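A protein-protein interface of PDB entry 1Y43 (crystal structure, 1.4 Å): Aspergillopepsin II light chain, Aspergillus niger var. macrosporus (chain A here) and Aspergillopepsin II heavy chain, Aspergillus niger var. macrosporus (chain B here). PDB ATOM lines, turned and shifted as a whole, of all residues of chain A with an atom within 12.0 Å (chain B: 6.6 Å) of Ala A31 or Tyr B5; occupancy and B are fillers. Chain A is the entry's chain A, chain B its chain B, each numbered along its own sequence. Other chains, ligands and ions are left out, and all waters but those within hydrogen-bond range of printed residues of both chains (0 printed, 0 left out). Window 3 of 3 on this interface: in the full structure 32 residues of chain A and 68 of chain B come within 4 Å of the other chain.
OH of Tyr B5 lies within hydrogen-bond range of OE2 of Glu B3 (3.4 Å). The backbone NH (N) of Phe B29 sits at hydrogen-bond distance from the backbone carbonyl oxygen (O) of Ala B7. N of Tyr B31 lies within hydrogen-bond range of O of Tyr B5 (2.8 Å). The backbone carbonyl oxygen (O) of Cys B6 lies within hydrogen-bond range of the backbone NH (N) of Ala B122, 3.0 Å away. The side-chain sulfur of Cys B30 forms a disulfide with the side-chain sulfur of Cys B6, at 2.0 Å.
Hydrophobic or aromatic side chains of chain B that line the printed part of chain A: Tyr B5, Phe B29, Tyr B31, Ala B122 and Tyr B172. Printed residues of chain A that touch a printed residue of chain B: Pro A27, Ser A28, Val A29, Ser A30, Ala A31 and Gly A32. Along chain A the printed residues that touch a printed residue of chain B span positions 27 to 32. Among the printed residues, 15 pairs touch across the chains.
The backbone NH (N) of Ser A30 lies within hydrogen-bond range of the backbone carbonyl oxygen (O) of Asp B123, 2.9 Å away.
Of the printed residues of chain B, Ala A31 touches Tyr B5, Tyr B31 and Asp B123. Tyr B5 touches just these residues of chain A: Ala A31 (3.6 Å) and Gly A32 (3.4 Å). No residue of chain A comes within 4 Å of Glu B3. No residue of chain A comes within 4 Å of Glu B4. No residue of chain A comes within 4 Å of Cys B6. Cys B30 touches just one residue of chain A: Val A29 (3.9 Å). Tyr B31 touches just these residues of chain A: Val A29 (3.8 Å), Ser A30 (3.9 Å) and Ala A31 (3.7 Å). No residue of chain A comes within 4 Å of Ala B120. Of chain A, only Ser A30 comes within 4 Å of Ala B122. Printed residues of chain A within 4 Å of Phe B29: Pro A27 (3.8 Å) and Val A29 (3.7 Å). Of the printed residues of chain B, Ser A28 touches Asp B123. Of the printed residues of chain A, Phe B121 touches Gly A32 (3.3 Å). Of the printed residues of chain A, Tyr B172 touches Gly A32. Of the printed residues of chain B, Pro A27 touches Phe B29 (3.8 Å). Glu B32 touches none of the printed residues of chain A. Val A26 touches none of the printed residues of chain B. The nearest residue of chain A that does not touch Tyr B5 is Ser A30 (4.3 Å). The nearest printed residue of chain B that does not touch Gly A32 is Asp B123 (4.03 Å).
Among the printed residues, merely in contact across the chains: Pro A27 with Phe B29, Ser A28 with Asp B123, Val A29 with Phe B29, Val A29 with Cys B30, Val A29 with Tyr B31, Val A29 with Asp B123, Ser A30 with Tyr B31, Ser A30 with Ala B122, Ala A31 with Tyr B5, Ala A31 with Tyr B31, Ala A31 with Asp B123, Gly A32 with Tyr B5, Gly A32 with Phe B121 and Gly A32 with Tyr B172.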
ATOM      1  N   VAL A  26      15.484   9.292  33.612  1.00  0.00           N
ATOM      2  CA  VAL A  26      14.767   8.844  32.431  1.00  0.00           C
ATOM      3  C   VAL A  26      13.349   9.378  32.521  1.00  0.00           C
ATOM      4  O   VAL A  26      12.608   9.048  33.457  1.00  0.00           O
ATOM      5  CB  VAL A  26      14.781   7.323  32.327  1.00  0.00           C
ATOM      6  CG1 VAL A  26      14.027   6.884  31.095  1.00  0.00           C
ATOM      7  CG2 VAL A  26      16.224   6.827  32.242  1.00  0.00           C
ATOM      8  N   PRO A  27      12.940  10.177  31.527  1.00  0.00           N
ATOM      9  CA  PRO A  27      11.601  10.764  31.521  1.00  0.00           C
ATOM     10  C   PRO A  27      10.442   9.866  31.132  1.00  0.00           C
ATOM     11  O   PRO A  27      10.617   8.791  30.558  1.00  0.00           O
ATOM     12  CB  PRO A  27      11.751  11.888  30.505  1.00  0.00           C
ATOM     13  CG  PRO A  27      12.615  11.253  29.465  1.00  0.00           C
ATOM     14  CD  PRO A  27      13.693  10.586  30.323  1.00  0.00           C
ATOM     15  N   SER A  28       9.252  10.357  31.450  1.00  0.00           N
ATOM     16  CA  SER A  28       7.992   9.713  31.112  1.00  0.00           C
ATOM     17  C   SER A  28       7.625  10.307  29.744  1.00  0.00           C
ATOM     18  O   SER A  28       7.574  11.532  29.594  1.00  0.00           O
ATOM     19  CB  SER A  28       6.933  10.097  32.147  1.00  0.00           C
ATOM     20  OG  SER A  28       5.747   9.356  31.932  1.00  0.00           O
ATOM     21  N   VAL A  29       7.400   9.450  28.749  1.00  0.00           N
ATOM     22  CA  VAL A  29       7.067   9.925  27.406  1.00  0.00           C
ATOM     23  C   VAL A  29       5.644   9.610  26.964  1.00  0.00           C
ATOM     24  O   VAL A  29       5.063   8.577  27.328  1.00  0.00           O
ATOM     25  CB  VAL A  29       8.036   9.375  26.316  1.00  0.00           C
ATOM     26  CG1 VAL A  29       9.397  10.020  26.447  1.00  0.00           C
ATOM     27  CG2 VAL A  29       8.155   7.856  26.413  1.00  0.00           C
ATOM     28  N   SER A  30       5.090  10.527  26.183  1.00  0.00           N
ATOM     29  CA  SER A  30       3.755  10.391  25.633  1.00  0.00           C
ATOM     30  C   SER A  30       3.783  10.912  24.193  1.00  0.00           C
ATOM     31  O   SER A  30       4.834  11.336  23.691  1.00  0.00           O
ATOM     32  CB  SER A  30       2.744  11.170  26.484  1.00  0.00           C
ATOM     33  OG  SER A  30       3.065  12.546  26.529  1.00  0.00           O
ATOM     34  N   ALA A  31       2.637  10.859  23.523  1.00  0.00           N
ATOM     35  CA  ALA A  31       2.533  11.329  22.148  1.00  0.00           C
ATOM     36  C   ALA A  31       2.814  12.818  22.039  1.00  0.00           C
ATOM     37  O   ALA A  31       2.429  13.595  22.911  1.00  0.00           O
ATOM     38  CB  ALA A  31       1.140  11.033  21.605  1.00  0.00           C
ATOM     39  N   GLY A  32       3.513  13.193  20.976  1.00  0.00           N
ATOM     40  CA  GLY A  32       3.799  14.593  20.734  1.00  0.00           C
ATOM     41  C   GLY A  32       2.616  15.237  20.029  1.00  0.00           C
ATOM     42  O   GLY A  32       1.677  14.500  19.649  1.00  0.00           O
ATOM     43  N   GLU B   3       0.888   5.306  15.752  1.00  0.00           N
ATOM     44  CA  GLU B   3       2.119   6.095  15.435  1.00  0.00           C
ATOM     45  C   GLU B   3       3.093   6.034  16.612  1.00  0.00           C
ATOM     46  O   GLU B   3       2.671   5.990  17.762  1.00  0.00           O
ATOM     47  CB  GLU B   3       1.741   7.547  15.137  1.00  0.00           C
ATOM     48  CG  GLU B   3       2.877   8.394  14.594  1.00  0.00           C
ATOM     49  CD  GLU B   3       2.399   9.757  14.130  1.00  0.00           C
ATOM     50  OE1 GLU B   3       1.303   9.848  13.525  1.00  0.00           O
ATOM     51  OE2 GLU B   3       3.121  10.747  14.365  1.00  0.00           O
ATOM     52  N   GLU B   4       4.386   6.012  16.324  1.00  0.00           N
ATOM     53  CA  GLU B   4       5.389   5.950  17.382  1.00  0.00           C
ATOM     54  C   GLU B   4       6.138   7.268  17.486  1.00  0.00           C
ATOM     55  O   GLU B   4       6.542   7.840  16.478  1.00  0.00           O
ATOM     56  CB  GLU B   4       6.385   4.820  17.133  1.00  0.00           C
ATOM     57  CG  GLU B   4       7.362   4.644  18.274  1.00  0.00           C
ATOM     58  CD  GLU B   4       8.183   3.378  18.178  1.00  0.00           C
ATOM     59  OE1 GLU B   4       7.979   2.555  17.249  1.00  0.00           O
ATOM     60  OE2 GLU B   4       9.046   3.205  19.055  1.00  0.00           O
ATOM     61  N   TYR B   5       6.327   7.729  18.712  1.00  0.00           N
ATOM     62  CA  TYR B   5       7.017   8.980  18.979  1.00  0.00           C
ATOM     63  C   TYR B   5       8.255   8.690  19.798  1.00  0.00           C
ATOM     64  O   TYR B   5       8.178   7.923  20.750  1.00  0.00           O
ATOM     65  CB  TYR B   5       6.115   9.883  19.810  1.00  0.00           C
ATOM     66  CG  TYR B   5       4.818  10.195  19.145  1.00  0.00           C
ATOM     67  CD1 TYR B   5       3.744   9.317  19.229  1.00  0.00           C
ATOM     68  CD2 TYR B   5       4.668  11.364  18.414  1.00  0.00           C
ATOM     69  CE1 TYR B   5       2.544   9.598  18.596  1.00  0.00           C
ATOM     70  CE2 TYR B   5       3.476  11.661  17.774  1.00  0.00           C
ATOM     71  CZ  TYR B   5       2.419  10.776  17.868  1.00  0.00           C
ATOM     72  OH  TYR B   5       1.245  11.076  17.209  1.00  0.00           O
ATOM     73  N   CYS B   6       9.371   9.330  19.466  1.00  0.00           N
ATOM     74  CA  CYS B   6      10.611   9.114  20.219  1.00  0.00           C
ATOM     75  C   CYS B   6      11.374  10.414  20.419  1.00  0.00           C
ATOM     76  O   CYS B   6      11.084  11.438  19.795  1.00  0.00           O
ATOM     77  CB  CYS B   6      11.556   8.165  19.464  1.00  0.00           C
ATOM     78  SG  CYS B   6      10.932   6.510  19.029  1.00  0.00           S
ATOM     79  N   ALA B   7      12.403  10.328  21.258  1.00  0.00           N
ATOM     80  CA  ALA B   7      13.315  11.431  21.533  1.00  0.00           C
ATOM     81  C   ALA B   7      14.569  10.764  22.099  1.00  0.00           C
ATOM     82  O   ALA B   7      14.533   9.591  22.456  1.00  0.00           O
ATOM     83  CB  ALA B   7      12.705  12.393  22.548  1.00  0.00           C
ATOM     84  N   PHE B  29      14.093   7.184  24.087  1.00  0.00           N
ATOM     85  CA  PHE B  29      12.837   6.878  24.780  1.00  0.00           C
ATOM     86  C   PHE B  29      11.736   6.964  23.746  1.00  0.00           C
ATOM     87  O   PHE B  29      11.616   7.972  23.058  1.00  0.00           O
ATOM     88  CB  PHE B  29      12.498   7.819  25.958  1.00  0.00           C
ATOM     89  CG  PHE B  29      13.393   9.010  26.091  1.00  0.00           C
ATOM     90  CD1 PHE B  29      14.583   8.916  26.803  1.00  0.00           C
ATOM     91  CD2 PHE B  29      13.018  10.242  25.551  1.00  0.00           C
ATOM     92  CE1 PHE B  29      15.399  10.034  26.981  1.00  0.00           C
ATOM     93  CE2 PHE B  29      13.819  11.373  25.717  1.00  0.00           C
ATOM     94  CZ  PHE B  29      15.011  11.267  26.435  1.00  0.00           C
ATOM     95  N   CYS B  30      10.986   5.881  23.589  1.00  0.00           N
ATOM     96  CA  CYS B  30       9.898   5.838  22.624  1.00  0.00           C
ATOM     97  C   CYS B  30       8.568   5.443  23.230  1.00  0.00           C
ATOM     98  O   CYS B  30       8.513   4.674  24.189  1.00  0.00           O
ATOM     99  CB  CYS B  30      10.222   4.877  21.495  1.00  0.00           C
ATOM    100  SG  CYS B  30      11.669   5.317  20.491  1.00  0.00           S
ATOM    101  N   TYR B  31       7.504   5.967  22.630  1.00  0.00           N
ATOM    102  CA  TYR B  31       6.144   5.712  23.046  1.00  0.00           C
ATOM    103  C   TYR B  31       5.317   5.263  21.844  1.00  0.00           C
ATOM    104  O   TYR B  31       5.405   5.853  20.762  1.00  0.00           O
ATOM    105  CB  TYR B  31       5.507   6.986  23.600  1.00  0.00           C
ATOM    106  CG  TYR B  31       4.026   6.806  23.817  1.00  0.00           C
ATOM    107  CD1 TYR B  31       3.557   6.067  24.895  1.00  0.00           C
ATOM    108  CD2 TYR B  31       3.096   7.270  22.882  1.00  0.00           C
ATOM    109  CE1 TYR B  31       2.205   5.783  25.042  1.00  0.00           C
ATOM    110  CE2 TYR B  31       1.727   6.985  23.021  1.00  0.00           C
ATOM    111  CZ  TYR B  31       1.299   6.240  24.105  1.00  0.00           C
ATOM    112  OH  TYR B  31      -0.033   5.925  24.273  1.00  0.00           O
ATOM    113  N   GLU B  32       4.477   4.260  22.061  1.00  0.00           N
ATOM    114  CA  GLU B  32       3.598   3.774  21.018  1.00  0.00           C
ATOM    115  C   GLU B  32       2.443   3.011  21.650  1.00  0.00           C
ATOM    116  O   GLU B  32       2.661   2.056  22.377  1.00  0.00           O
ATOM    117  CB  GLU B  32       4.356   2.853  20.063  1.00  0.00           C
ATOM    118  CG  GLU B  32       3.561   2.499  18.837  1.00  0.00           C
ATOM    119  CD  GLU B  32       3.759   1.064  18.412  1.00  0.00           C
ATOM    120  OE1 GLU B  32       4.928   0.664  18.195  1.00  0.00           O
ATOM    121  OE2 GLU B  32       2.742   0.339  18.284  1.00  0.00           O
ATOM    122  N   VAL B 119      12.122  11.240  13.253  1.00  0.00           N
ATOM    123  CA  VAL B 119      11.113  10.459  13.948  1.00  0.00           C
ATOM    124  C   VAL B 119      10.089  11.415  14.590  1.00  0.00           C
ATOM    125  O   VAL B 119      10.415  12.556  14.928  1.00  0.00           O
ATOM    126  CB  VAL B 119      11.779   9.540  15.031  1.00  0.00           C
ATOM    127  CG1 VAL B 119      12.334  10.350  16.185  1.00  0.00           C
ATOM    128  CG2 VAL B 119      10.817   8.469  15.505  1.00  0.00           C
ATOM    129  N   ALA B 120       8.830  10.991  14.662  1.00  0.00           N
ATOM    130  CA  ALA B 120       7.798  11.820  15.286  1.00  0.00           C
ATOM    131  C   ALA B 120       8.334  12.076  16.686  1.00  0.00           C
ATOM    132  O   ALA B 120       8.769  11.138  17.371  1.00  0.00           O
ATOM    133  CB  ALA B 120       6.474  11.076  15.338  1.00  0.00           C
ATOM    134  N   PHE B 121       8.332  13.343  17.080  1.00  0.00           N
ATOM    135  CA  PHE B 121       8.892  13.779  18.353  1.00  0.00           C
ATOM    136  C   PHE B 121       8.000  13.573  19.581  1.00  0.00           C
ATOM    137  O   PHE B 121       6.911  14.126  19.674  1.00  0.00           O
ATOM    138  CB  PHE B 121       9.289  15.242  18.201  1.00  0.00           C
ATOM    139  CG  PHE B 121      10.323  15.699  19.173  1.00  0.00           C
ATOM    140  CD1 PHE B 121      11.457  14.930  19.442  1.00  0.00           C
ATOM    141  CD2 PHE B 121      10.183  16.929  19.793  1.00  0.00           C
ATOM    142  CE1 PHE B 121      12.446  15.398  20.324  1.00  0.00           C
ATOM    143  CE2 PHE B 121      11.153  17.409  20.672  1.00  0.00           C
ATOM    144  CZ  PHE B 121      12.288  16.646  20.940  1.00  0.00           C
ATOM    145  N   ALA B 122       8.494  12.786  20.535  1.00  0.00           N
ATOM    146  CA  ALA B 122       7.754  12.481  21.755  1.00  0.00           C
ATOM    147  C   ALA B 122       7.689  13.628  22.773  1.00  0.00           C
ATOM    148  O   ALA B 122       8.600  14.453  22.860  1.00  0.00           O
ATOM    149  CB  ALA B 122       8.353  11.248  22.424  1.00  0.00           C
ATOM    150  N   ASP B 123       6.591  13.681  23.526  1.00  0.00           N
ATOM    151  CA  ASP B 123       6.455  14.660  24.605  1.00  0.00           C
ATOM    152  C   ASP B 123       7.093  13.946  25.805  1.00  0.00           C
ATOM    153  O   ASP B 123       6.520  13.017  26.372  1.00  0.00           O
ATOM    154  CB  ASP B 123       4.988  14.969  24.900  1.00  0.00           C
ATOM    155  CG  ASP B 123       4.815  15.971  26.035  1.00  0.00           C
ATOM    156  OD1 ASP B 123       5.789  16.266  26.766  1.00  0.00           O
ATOM    157  OD2 ASP B 123       3.692  16.475  26.198  1.00  0.00           O
ATOM    158  N   TYR B 172       9.658  20.135  26.915  1.00  0.00           N
ATOM    159  CA  TYR B 172       8.851  19.978  25.718  1.00  0.00           C
ATOM    160  C   TYR B 172       7.735  21.031  25.714  1.00  0.00           C
ATOM    161  O   TYR B 172       7.098  21.286  26.736  1.00  0.00           O
ATOM    162  CB  TYR B 172       8.271  18.561  25.649  1.00  0.00           C
ATOM    163  CG  TYR B 172       7.387  18.336  24.435  1.00  0.00           C
ATOM    164  CD1 TYR B 172       7.924  17.886  23.241  1.00  0.00           C
ATOM    165  CD2 TYR B 172       6.019  18.610  24.480  1.00  0.00           C
ATOM    166  CE1 TYR B 172       7.138  17.713  22.109  1.00  0.00           C
ATOM    167  CE2 TYR B 172       5.214  18.443  23.365  1.00  0.00           C
ATOM    168  CZ  TYR B 172       5.791  17.990  22.173  1.00  0.00           C
ATOM    169  OH  TYR B 172       5.021  17.807  21.053  1.00  0.00           O
